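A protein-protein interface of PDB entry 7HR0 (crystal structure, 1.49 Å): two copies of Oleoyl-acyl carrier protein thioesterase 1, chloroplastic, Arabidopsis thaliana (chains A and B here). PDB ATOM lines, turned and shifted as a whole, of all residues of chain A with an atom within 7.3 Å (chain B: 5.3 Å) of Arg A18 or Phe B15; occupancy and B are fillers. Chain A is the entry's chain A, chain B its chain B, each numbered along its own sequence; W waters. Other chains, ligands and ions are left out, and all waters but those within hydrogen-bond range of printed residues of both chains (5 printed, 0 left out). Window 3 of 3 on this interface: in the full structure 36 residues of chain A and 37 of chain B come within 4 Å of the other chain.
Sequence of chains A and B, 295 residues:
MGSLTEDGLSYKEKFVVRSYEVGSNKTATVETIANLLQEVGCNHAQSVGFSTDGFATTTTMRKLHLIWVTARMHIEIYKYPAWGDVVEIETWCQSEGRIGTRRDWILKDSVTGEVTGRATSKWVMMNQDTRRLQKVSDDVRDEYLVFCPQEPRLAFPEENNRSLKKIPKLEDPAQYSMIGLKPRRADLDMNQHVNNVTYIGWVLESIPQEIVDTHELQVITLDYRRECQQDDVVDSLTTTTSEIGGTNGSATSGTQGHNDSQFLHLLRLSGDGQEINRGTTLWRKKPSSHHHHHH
OE1 of Glu B39 sits at hydrogen-bond distance from N of Ser A19 (2.8 Å). OE2 of Glu B21 lies within salt-bridge range of NH1 of Arg A18 (2.9 Å). NH1 of Arg B18 lies within salt-bridge range of OE2 of Glu A21, at 2.9 Å.
The backbone carbonyl oxygen of Glu A21 sits at hydrogen-bond distance from the side-chain hydroxyl of Thr A32, at 2.8 Å. The backbone NH (N) of Arg B18 lies within hydrogen-bond range of the side-chain carboxylate (OE1) of Glu B21. The guanidinium group of Arg A18 sits at hydrogen-bond distance from the side-chain hydroxyl of Tyr A20, at 2.9 Å. N of Phe B15 lies within hydrogen-bond range of O of Val B87 (2.9 Å). The backbone NH (N) of Arg A18 lies within hydrogen-bond range of the side-chain carboxylate (OE1) of Glu A21.
Among the printed residues, merely in contact across the chains: Phe A15 with Arg B18 (3.7 Å), Arg A18 with Phe B15 (3.7 Å), Arg A18 with Arg B18 (3.5 Å), Arg A18 with Leu B36 (3.6 Å), Arg A18 with Glu B39 (3.6 Å), Tyr A20 with Glu B21 (3.9 Å) and Leu A36 with Arg B18 (3.6 Å).
Printed residues of chain B within 4 Å of Phe A15: Arg B18 (3.7 Å). Arg A18 touches five residues of chain B. Printed residues of chain B within 4 Å of Glu A21: Arg B18 (2.9 Å). Phe B15 touches one residue of chain A. Val B17 touches none of the printed residues of chain A. Of the printed residues of chain A, Arg B18 touches Phe A15 (3.7 Å), Arg A18 (3.5 Å), Glu A21 (2.9 Å) and Leu A36 (3.6 Å). Ile B89 touches none of the printed residues of chain A. The nearest residue of chain B that does not touch Arg A18 is Val B16 (4.6 Å). The nearest residue of chain A that does not touch Phe B15 is Tyr A20 (6.7 Å). The nearest printed residue of chain B that does not touch Phe A15 is Val B16 (7.7 Å).
Printed residues of chain B that touch a printed residue of chain A: Phe B15, Arg B18, Glu B21, Leu B36 and Glu B39. Among the printed residues, 10 pairs touch across the chains. Among the printed residues, Asp or Glu carboxylates within 4 Å of a Lys or Arg side-chain nitrogen of the other chain: Arg A18 with Glu B21 and Glu A21 with Arg B18.
Phe A15 touches Arg B18, and with the chains exchanged Arg A18 touches Phe B15. Arg B18 touches its own counterpart, Arg A18. Arg A18 touches Glu B21, and with the chains exchanged Glu A21 touches Arg B18. Arg A18 touches Leu B36, and with the chains exchanged Leu A36 touches Arg B18. Positions printed for both chains: 15, 16, 17, 18, 21, 36 and 85. Of the 10 pairs that touch across the chains among the printed residues, 7 have their exchanged pair printed and touching as well.
Water W4 lies within hydrogen-bond range of OH of Tyr A20 (2.6 Å) and OE2 of Glu B21 (2.6 Å). Water W3 lies within hydrogen-bond range of O of Val A16, OE1 of Glu A21 and NH2 of Arg B18. Water W1 lies within hydrogen-bond range of OE1 of Glu B21 (2.8 Å), NH2 of Arg A18 (2.8 Å) and O of Val B16 (2.8 Å). Water W2 lies within hydrogen-bond range of OE2 of Glu B39 (2.8 Å) and O of Val A17 (2.8 Å). Water W5 bridges the indole nitrogen of Trp A83 and the side-chain carboxylate of Glu B39.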
ATOM      1  N   PHE A  15     -17.366  26.223  31.156  1.00  0.00           N
ATOM      2  CA  PHE A  15     -16.947  25.734  29.848  1.00  0.00           C
ATOM      3  C   PHE A  15     -15.583  26.331  29.493  1.00  0.00           C
ATOM      4  O   PHE A  15     -15.368  27.536  29.676  1.00  0.00           O
ATOM      5  CB  PHE A  15     -17.950  26.206  28.785  1.00  0.00           C
ATOM      6  CG  PHE A  15     -19.340  25.670  29.005  1.00  0.00           C
ATOM      7  CD1 PHE A  15     -19.715  24.438  28.499  1.00  0.00           C
ATOM      8  CD2 PHE A  15     -20.289  26.420  29.685  1.00  0.00           C
ATOM      9  CE1 PHE A  15     -21.013  23.942  28.706  1.00  0.00           C
ATOM     10  CE2 PHE A  15     -21.579  25.944  29.867  1.00  0.00           C
ATOM     11  CZ  PHE A  15     -21.938  24.713  29.371  1.00  0.00           C
ATOM     12  N   VAL A  16     -14.688  25.509  28.951  1.00  0.00           N
ATOM     13  CA  VAL A  16     -13.395  25.985  28.454  1.00  0.00           C
ATOM     14  C   VAL A  16     -13.574  26.259  26.946  1.00  0.00           C
ATOM     15  O   VAL A  16     -13.943  25.329  26.208  1.00  0.00           O
ATOM     16  CB  VAL A  16     -12.260  24.959  28.678  1.00  0.00           C
ATOM     17  CG1 VAL A  16     -10.963  25.475  28.073  1.00  0.00           C
ATOM     18  CG2 VAL A  16     -12.065  24.680  30.171  1.00  0.00           C
ATOM     19  N   VAL A  17     -13.360  27.505  26.491  1.00  0.00           N
ATOM     20  CA  VAL A  17     -13.564  27.819  25.056  1.00  0.00           C
ATOM     21  C   VAL A  17     -12.595  27.051  24.146  1.00  0.00           C
ATOM     22  O   VAL A  17     -11.381  27.044  24.385  1.00  0.00           O
ATOM     23  CB  VAL A  17     -13.532  29.349  24.791  1.00  0.00           C
ATOM     24  CG1 VAL A  17     -13.768  29.670  23.308  1.00  0.00           C
ATOM     25  CG2 VAL A  17     -14.561  30.050  25.677  1.00  0.00           C
ATOM     26  N   ARG A  18     -13.149  26.357  23.129  1.00  0.00           N
ATOM     27  CA  ARG A  18     -12.395  25.509  22.213  1.00  0.00           C
ATOM     28  C   ARG A  18     -11.821  26.280  21.023  1.00  0.00           C
ATOM     29  O   ARG A  18     -12.388  27.296  20.583  1.00  0.00           O
ATOM     30  CB  ARG A  18     -13.320  24.363  21.720  1.00  0.00           C
ATOM     31  CG  ARG A  18     -13.761  23.467  22.910  1.00  0.00           C
ATOM     32  CD  ARG A  18     -14.716  22.359  22.496  1.00  0.00           C
ATOM     33  NE  ARG A  18     -15.100  21.517  23.631  1.00  0.00           N
ATOM     34  CZ  ARG A  18     -16.030  20.558  23.563  1.00  0.00           C
ATOM     35  NH1 ARG A  18     -16.693  20.338  22.421  1.00  0.00           N
ATOM     36  NH2 ARG A  18     -16.314  19.824  24.636  1.00  0.00           N
ATOM     37  N   SER A  19     -10.767  25.711  20.415  1.00  0.00           N
ATOM     38  CA  SER A  19     -10.095  26.309  19.254  1.00  0.00           C
ATOM     39  C   SER A  19     -11.074  26.585  18.112  1.00  0.00           C
ATOM     40  O   SER A  19     -11.020  27.648  17.480  1.00  0.00           O
ATOM     41  CB  SER A  19      -8.999  25.363  18.746  1.00  0.00           C
ATOM     42  OG  SER A  19      -9.517  24.081  18.393  1.00  0.00           O
ATOM     43  N   TYR A  20     -11.955  25.607  17.813  1.00  0.00           N
ATOM     44  CA  TYR A  20     -12.863  25.766  16.666  1.00  0.00           C
ATOM     45  C   TYR A  20     -14.105  26.644  16.943  1.00  0.00           C
ATOM     46  O   TYR A  20     -14.878  26.938  16.034  1.00  0.00           O
ATOM     47  CB  TYR A  20     -13.267  24.386  16.092  1.00  0.00           C
ATOM     48  CG  TYR A  20     -14.051  23.525  17.065  1.00  0.00           C
ATOM     49  CD1 TYR A  20     -15.427  23.681  17.210  1.00  0.00           C
ATOM     50  CD2 TYR A  20     -13.418  22.563  17.844  1.00  0.00           C
ATOM     51  CE1 TYR A  20     -16.155  22.882  18.088  1.00  0.00           C
ATOM     52  CE2 TYR A  20     -14.130  21.774  18.743  1.00  0.00           C
ATOM     53  CZ  TYR A  20     -15.505  21.922  18.847  1.00  0.00           C
ATOM     54  OH  TYR A  20     -16.219  21.108  19.690  1.00  0.00           O
ATOM     55  N   GLU A  21     -14.255  27.079  18.183  1.00  0.00           N
ATOM     56  CA  GLU A  21     -15.372  27.884  18.628  1.00  0.00           C
ATOM     57  C   GLU A  21     -15.126  29.407  18.473  1.00  0.00           C
ATOM     58  O   GLU A  21     -16.044  30.181  18.758  1.00  0.00           O
ATOM     59  CB  GLU A  21     -15.645  27.545  20.111  1.00  0.00           C
ATOM     60  CG  GLU A  21     -16.391  26.215  20.318  1.00  0.00           C
ATOM     61  CD  GLU A  21     -16.643  25.821  21.776  1.00  0.00           C
ATOM     62  OE1 GLU A  21     -15.971  26.365  22.683  1.00  0.00           O
ATOM     63  OE2 GLU A  21     -17.481  24.918  22.010  1.00  0.00           O
ATOM     64  N   VAL A  22     -13.871  29.816  18.147  1.00  0.00           N
ATOM     65  CA  VAL A  22     -13.543  31.229  18.070  1.00  0.00           C
ATOM     66  C   VAL A  22     -13.512  31.760  16.651  1.00  0.00           C
ATOM     67  O   VAL A  22     -13.251  31.010  15.718  1.00  0.00           O
ATOM     68  CB  VAL A  22     -12.218  31.575  18.823  1.00  0.00           C
ATOM     69  CG1 VAL A  22     -12.220  30.972  20.222  1.00  0.00           C
ATOM     70  CG2 VAL A  22     -11.008  31.106  18.048  1.00  0.00           C
ATOM     71  N   GLY A  23     -13.759  33.055  16.520  1.00  0.00           N
ATOM     72  CA  GLY A  23     -13.701  33.738  15.223  1.00  0.00           C
ATOM     73  C   GLY A  23     -12.390  34.476  15.002  1.00  0.00           C
ATOM     74  O   GLY A  23     -11.371  34.119  15.599  1.00  0.00           O
ATOM     75  N   THR A  27     -11.798  35.172  19.806  1.00  0.00           N
ATOM     76  CA  THR A  27     -12.772  35.099  20.889  1.00  0.00           C
ATOM     77  C   THR A  27     -14.011  34.314  20.372  1.00  0.00           C
ATOM     78  O   THR A  27     -14.215  34.214  19.153  1.00  0.00           O
ATOM     79  CB  THR A  27     -13.142  36.478  21.461  1.00  0.00           C
ATOM     80  OG1 THR A  27     -13.840  37.252  20.488  1.00  0.00           O
ATOM     81  CG2 THR A  27     -11.916  37.244  21.979  1.00  0.00           C
ATOM     82  N   ALA A  28     -14.778  33.732  21.291  1.00  0.00           N
ATOM     83  CA  ALA A  28     -15.947  32.902  20.974  1.00  0.00           C
ATOM     84  C   ALA A  28     -16.947  33.659  20.112  1.00  0.00           C
ATOM     85  O   ALA A  28     -17.173  34.854  20.341  1.00  0.00           O
ATOM     86  CB  ALA A  28     -16.623  32.422  22.255  1.00  0.00           C
ATOM     87  N   THR A  32     -21.227  30.269  19.133  1.00  0.00           N
ATOM     88  CA  THR A  32     -20.647  29.426  20.210  1.00  0.00           C
ATOM     89  C   THR A  32     -21.325  29.749  21.566  1.00  0.00           C
ATOM     90  O   THR A  32     -21.791  28.833  22.269  1.00  0.00           O
ATOM     91  CB  THR A  32     -19.138  29.634  20.328  1.00  0.00           C
ATOM     92  OG1 THR A  32     -18.552  29.004  19.175  1.00  0.00           O
ATOM     93  CG2 THR A  32     -18.551  29.072  21.690  1.00  0.00           C
ATOM     94  N   LEU A  36     -23.554  27.238  24.046  1.00  0.00           N
ATOM     95  CA  LEU A  36     -23.269  27.017  25.480  1.00  0.00           C
ATOM     96  C   LEU A  36     -24.523  27.291  26.318  1.00  0.00           C
ATOM     97  O   LEU A  36     -24.826  26.563  27.279  1.00  0.00           O
ATOM     98  CB  LEU A  36     -22.101  27.879  25.962  1.00  0.00           C
ATOM     99  CG  LEU A  36     -20.745  27.702  25.231  1.00  0.00           C
ATOM    100  CD1 LEU A  36     -19.658  28.548  25.895  1.00  0.00           C
ATOM    101  CD2 LEU A  36     -20.323  26.232  25.138  1.00  0.00           C
ATOM    102  N   ALA A  82     -11.980  34.411  25.246  1.00  0.00           N
ATOM    103  CA  ALA A  82     -10.973  33.985  24.304  1.00  0.00           C
ATOM    104  C   ALA A  82     -10.781  32.468  24.364  1.00  0.00           C
ATOM    105  O   ALA A  82     -11.194  31.794  25.313  1.00  0.00           O
ATOM    106  CB  ALA A  82      -9.640  34.712  24.595  1.00  0.00           C
ATOM    107  N   TRP A  83     -10.145  31.919  23.333  1.00  0.00           N
ATOM    108  CA  TRP A  83      -9.765  30.523  23.239  1.00  0.00           C
ATOM    109  C   TRP A  83      -8.980  30.084  24.521  1.00  0.00           C
ATOM    110  O   TRP A  83      -8.023  30.771  24.927  1.00  0.00           O
ATOM    111  CB  TRP A  83      -8.898  30.484  21.989  1.00  0.00           C
ATOM    112  CG  TRP A  83      -8.162  29.242  21.694  1.00  0.00           C
ATOM    113  CD1 TRP A  83      -8.440  27.982  22.124  1.00  0.00           C
ATOM    114  CD2 TRP A  83      -7.061  29.129  20.790  1.00  0.00           C
ATOM    115  NE1 TRP A  83      -7.512  27.105  21.630  1.00  0.00           N
ATOM    116  CE2 TRP A  83      -6.655  27.781  20.797  1.00  0.00           C
ATOM    117  CE3 TRP A  83      -6.333  30.052  20.031  1.00  0.00           C
ATOM    118  CZ2 TRP A  83      -5.594  27.317  20.014  1.00  0.00           C
ATOM    119  CZ3 TRP A  83      -5.273  29.591  19.261  1.00  0.00           C
ATOM    120  CH2 TRP A  83      -4.930  28.236  19.238  1.00  0.00           C
ATOM    121  N   GLY A  84      -9.448  29.035  25.201  1.00  0.00           N
ATOM    122  CA  GLY A  84      -8.792  28.570  26.418  1.00  0.00           C
ATOM    123  C   GLY A  84      -9.323  29.178  27.711  1.00  0.00           C
ATOM    124  O   GLY A  84      -9.076  28.639  28.788  1.00  0.00           O
ATOM    125  N   ASP A  85     -10.038  30.304  27.625  1.00  0.00           N
ATOM    126  CA  ASP A  85     -10.643  30.920  28.822  1.00  0.00           C
ATOM    127  C   ASP A  85     -11.807  30.074  29.361  1.00  0.00           C
ATOM    128  O   ASP A  85     -12.416  29.291  28.623  1.00  0.00           O
ATOM    129  CB  ASP A  85     -11.212  32.312  28.490  1.00  0.00           C
ATOM    130  CG  ASP A  85     -10.199  33.413  28.275  1.00  0.00           C
ATOM    131  OD1 ASP A  85      -8.990  33.165  28.502  1.00  0.00           O
ATOM    132  OD2 ASP A  85     -10.619  34.533  27.861  1.00  0.00           O
ATOM    133  N   GLU B  13      -6.949  14.193  26.763  1.00  0.00           N
ATOM    134  CA  GLU B  13      -7.995  15.092  27.226  1.00  0.00           C
ATOM    135  C   GLU B  13      -9.319  14.348  27.246  1.00  0.00           C
ATOM    136  O   GLU B  13      -9.564  13.509  26.379  1.00  0.00           O
ATOM    137  CB  GLU B  13      -8.107  16.330  26.292  1.00  0.00           C
ATOM    138  CG  GLU B  13      -9.096  17.388  26.761  1.00  0.00           C
ATOM    139  CD  GLU B  13      -9.021  18.705  25.991  1.00  0.00           C
ATOM    140  OE1 GLU B  13      -8.099  18.861  25.153  1.00  0.00           O
ATOM    141  OE2 GLU B  13      -9.879  19.588  26.242  1.00  0.00           O
ATOM    142  N   LYS B  14     -10.182  14.665  28.229  1.00  0.00           N
ATOM    143  CA  LYS B  14     -11.518  14.088  28.349  1.00  0.00           C
ATOM    144  C   LYS B  14     -12.560  15.150  27.940  1.00  0.00           C
ATOM    145  O   LYS B  14     -12.416  16.344  28.255  1.00  0.00           O
ATOM    146  CB  LYS B  14     -11.809  13.665  29.806  1.00  0.00           C
ATOM    147  CG  LYS B  14     -11.029  12.448  30.250  1.00  0.00           C
ATOM    148  CD  LYS B  14     -11.205  12.198  31.753  1.00  0.00           C
ATOM    149  CE  LYS B  14     -10.299  11.100  32.242  1.00  0.00           C
ATOM    150  NZ  LYS B  14     -10.118  11.131  33.721  1.00  0.00           N
ATOM    151  N   PHE B  15     -13.614  14.702  27.271  1.00  0.00           N
ATOM    152  CA  PHE B  15     -14.698  15.557  26.830  1.00  0.00           C
ATOM    153  C   PHE B  15     -16.039  14.952  27.240  1.00  0.00           C
ATOM    154  O   PHE B  15     -16.252  13.749  27.064  1.00  0.00           O
ATOM    155  CB  PHE B  15     -14.689  15.644  25.298  1.00  0.00           C
ATOM    156  CG  PHE B  15     -13.423  16.251  24.745  1.00  0.00           C
ATOM    157  CD1 PHE B  15     -13.299  17.628  24.597  1.00  0.00           C
ATOM    158  CD2 PHE B  15     -12.372  15.447  24.327  1.00  0.00           C
ATOM    159  CE1 PHE B  15     -12.120  18.188  24.085  1.00  0.00           C
ATOM    160  CE2 PHE B  15     -11.213  16.006  23.795  1.00  0.00           C
ATOM    161  CZ  PHE B  15     -11.098  17.368  23.669  1.00  0.00           C
ATOM    162  N   VAL B  16     -16.952  15.789  27.741  1.00  0.00           N
ATOM    163  CA  VAL B  16     -18.317  15.343  28.059  1.00  0.00           C
ATOM    164  C   VAL B  16     -19.178  15.655  26.817  1.00  0.00           C
ATOM    165  O   VAL B  16     -19.248  16.825  26.414  1.00  0.00           O
ATOM    166  CB  VAL B  16     -18.892  16.058  29.296  1.00  0.00           C
ATOM    167  CG1 VAL B  16     -20.333  15.620  29.528  1.00  0.00           C
ATOM    168  CG2 VAL B  16     -18.043  15.757  30.537  1.00  0.00           C
ATOM    169  N   VAL B  17     -19.800  14.640  26.203  1.00  0.00           N
ATOM    170  CA  VAL B  17     -20.611  14.888  24.979  1.00  0.00           C
ATOM    171  C   VAL B  17     -21.820  15.796  25.261  1.00  0.00           C
ATOM    172  O   VAL B  17     -22.580  15.553  26.209  1.00  0.00           O
ATOM    173  CB  VAL B  17     -21.015  13.574  24.274  1.00  0.00           C
ATOM    174  CG1 VAL B  17     -21.839  13.838  23.003  1.00  0.00           C
ATOM    175  CG2 VAL B  17     -19.769  12.739  23.972  1.00  0.00           C
ATOM    176  N   ARG B  18     -21.954  16.873  24.458  1.00  0.00           N
ATOM    177  CA  ARG B  18     -22.998  17.880  24.630  1.00  0.00           C
ATOM    178  C   ARG B  18     -24.301  17.525  23.910  1.00  0.00           C
ATOM    179  O   ARG B  18     -24.291  16.826  22.882  1.00  0.00           O
ATOM    180  CB  ARG B  18     -22.460  19.249  24.121  1.00  0.00           C
ATOM    181  CG  ARG B  18     -21.240  19.707  24.952  1.00  0.00           C
ATOM    182  CD  ARG B  18     -20.652  21.020  24.470  1.00  0.00           C
ATOM    183  NE  ARG B  18     -19.516  21.446  25.298  1.00  0.00           N
ATOM    184  CZ  ARG B  18     -18.730  22.488  24.988  1.00  0.00           C
ATOM    185  NH1 ARG B  18     -18.938  23.183  23.870  1.00  0.00           N
ATOM    186  NH2 ARG B  18     -17.733  22.836  25.791  1.00  0.00           N
ATOM    187  N   GLU B  21     -24.387  18.141  20.148  1.00  0.00           N
ATOM    188  CA  GLU B  21     -23.370  17.389  19.444  1.00  0.00           C
ATOM    189  C   GLU B  21     -23.866  16.002  18.952  1.00  0.00           C
ATOM    190  O   GLU B  21     -23.094  15.313  18.287  1.00  0.00           O
ATOM    191  CB  GLU B  21     -22.166  17.200  20.392  1.00  0.00           C
ATOM    192  CG  GLU B  21     -21.293  18.457  20.540  1.00  0.00           C
ATOM    193  CD  GLU B  21     -20.111  18.342  21.501  1.00  0.00           C
ATOM    194  OE1 GLU B  21     -20.096  17.425  22.360  1.00  0.00           O
ATOM    195  OE2 GLU B  21     -19.214  19.218  21.427  1.00  0.00           O
ATOM    196  N   LEU B  36     -13.639  17.167  18.101  1.00  0.00           N
ATOM    197  CA  LEU B  36     -12.903  16.818  19.341  1.00  0.00           C
ATOM    198  C   LEU B  36     -11.454  16.437  19.009  1.00  0.00           C
ATOM    199  O   LEU B  36     -10.510  16.810  19.729  1.00  0.00           O
ATOM    200  CB  LEU B  36     -13.600  15.689  20.115  1.00  0.00           C
ATOM    201  CG  LEU B  36     -15.059  15.928  20.551  1.00  0.00           C
ATOM    202  CD1 LEU B  36     -15.559  14.765  21.398  1.00  0.00           C
ATOM    203  CD2 LEU B  36     -15.247  17.253  21.270  1.00  0.00           C
ATOM    204  N   GLU B  39      -9.629  19.714  18.447  1.00  0.00           N
ATOM    205  CA  GLU B  39      -9.392  20.389  19.723  1.00  0.00           C
ATOM    206  C   GLU B  39      -8.252  19.766  20.518  1.00  0.00           C
ATOM    207  O   GLU B  39      -7.350  20.507  20.961  1.00  0.00           O
ATOM    208  CB  GLU B  39     -10.705  20.416  20.538  1.00  0.00           C
ATOM    209  CG  GLU B  39     -10.556  20.975  21.953  1.00  0.00           C
ATOM    210  CD  GLU B  39     -10.150  22.431  22.067  1.00  0.00           C
ATOM    211  OE1 GLU B  39      -9.979  23.091  21.016  1.00  0.00           O
ATOM    212  OE2 GLU B  39     -10.022  22.920  23.212  1.00  0.00           O
ATOM    213  N   VAL B  40      -8.260  18.426  20.697  1.00  0.00           N
ATOM    214  CA  VAL B  40      -7.172  17.817  21.475  1.00  0.00           C
ATOM    215  C   VAL B  40      -5.814  17.990  20.732  1.00  0.00           C
ATOM    216  O   VAL B  40      -4.774  18.236  21.380  1.00  0.00           O
ATOM    217  CB  VAL B  40      -7.476  16.379  21.932  1.00  0.00           C
ATOM    218  CG1 VAL B  40      -7.479  15.396  20.756  1.00  0.00           C
ATOM    219  CG2 VAL B  40      -6.465  15.942  23.001  1.00  0.00           C
ATOM    220  N   ASP B  85     -21.971  11.195  28.082  1.00  0.00           N
ATOM    221  CA  ASP B  85     -20.838  10.283  28.290  1.00  0.00           C
ATOM    222  C   ASP B  85     -19.495  11.030  28.225  1.00  0.00           C
ATOM    223  O   ASP B  85     -19.400  12.104  27.621  1.00  0.00           O
ATOM    224  CB  ASP B  85     -20.809   9.190  27.213  1.00  0.00           C
ATOM    225  CG  ASP B  85     -21.864   8.113  27.316  1.00  0.00           C
ATOM    226  OD1 ASP B  85     -22.606   8.099  28.328  1.00  0.00           O
ATOM    227  OD2 ASP B  85     -21.961   7.287  26.367  1.00  0.00           O
ATOM    228  N   VAL B  86     -18.433  10.430  28.797  1.00  0.00           N
ATOM    229  CA  VAL B  86     -17.110  11.051  28.773  1.00  0.00           C
ATOM    230  C   VAL B  86     -16.228  10.240  27.858  1.00  0.00           C
ATOM    231  O   VAL B  86     -16.093   9.026  28.079  1.00  0.00           O
ATOM    232  CB  VAL B  86     -16.515  11.080  30.207  1.00  0.00           C
ATOM    233  CG1 VAL B  86     -15.145  11.747  30.205  1.00  0.00           C
ATOM    234  CG2 VAL B  86     -17.473  11.798  31.176  1.00  0.00           C
ATOM    235  N   VAL B  87     -15.614  10.889  26.856  1.00  0.00           N
ATOM    236  CA  VAL B  87     -14.699  10.200  25.963  1.00  0.00           C
ATOM    237  C   VAL B  87     -13.284  10.732  26.254  1.00  0.00           C
ATOM    238  O   VAL B  87     -13.135  11.940  26.471  1.00  0.00           O
ATOM    239  CB  VAL B  87     -15.067  10.373  24.468  1.00  0.00           C
ATOM    240  CG1 VAL B  87     -15.184  11.848  24.100  1.00  0.00           C
ATOM    241  CG2 VAL B  87     -14.046   9.675  23.566  1.00  0.00           C
ATOM    242  N   GLU B  88     -12.280   9.844  26.347  1.00  0.00           N
ATOM    243  CA  GLU B  88     -10.910  10.309  26.560  1.00  0.00           C
ATOM    244  C   GLU B  88     -10.175  10.093  25.243  1.00  0.00           C
ATOM    245  O   GLU B  88     -10.294   9.022  24.645  1.00  0.00           O
ATOM    246  CB  GLU B  88     -10.164   9.529  27.664  1.00  0.00           C
ATOM    247  CG  GLU B  88      -8.789  10.157  27.942  1.00  0.00           C
ATOM    248  CD  GLU B  88      -8.044   9.606  29.147  1.00  0.00           C
ATOM    249  OE1 GLU B  88      -7.740   8.390  29.142  1.00  0.00           O
ATOM    250  OE2 GLU B  88      -7.735  10.394  30.075  1.00  0.00           O
ATOM    251  N   ILE B  89      -9.426  11.104  24.792  1.00  0.00           N
ATOM    252  CA  ILE B  89      -8.696  10.994  23.538  1.00  0.00           C
ATOM    253  C   ILE B  89      -7.230  11.261  23.791  1.00  0.00           C
ATOM    254  O   ILE B  89      -6.884  12.243  24.477  1.00  0.00           O
ATOM    255  CB  ILE B  89      -9.230  12.014  22.501  1.00  0.00           C
ATOM    256  CG1 ILE B  89     -10.790  11.881  22.385  1.00  0.00           C
ATOM    257  CG2 ILE B  89      -8.547  11.770  21.149  1.00  0.00           C
ATOM    258  CD1 ILE B  89     -11.461  12.901  21.382  1.00  0.00           C
HETATM  259  O   HOH W   1     -17.921  17.616  24.071  1.00  0.00           O
HETATM  260  O   HOH W   2      -9.179  25.290  24.390  1.00  0.00           O
HETATM  261  O   HOH W   3     -16.512  25.275  25.174  1.00  0.00           O
HETATM  262  O   HOH W   4     -18.840  21.089  19.601  1.00  0.00           O
HETATM  263  O   HOH W   5      -7.229  24.309  21.648  1.00  0.00           O
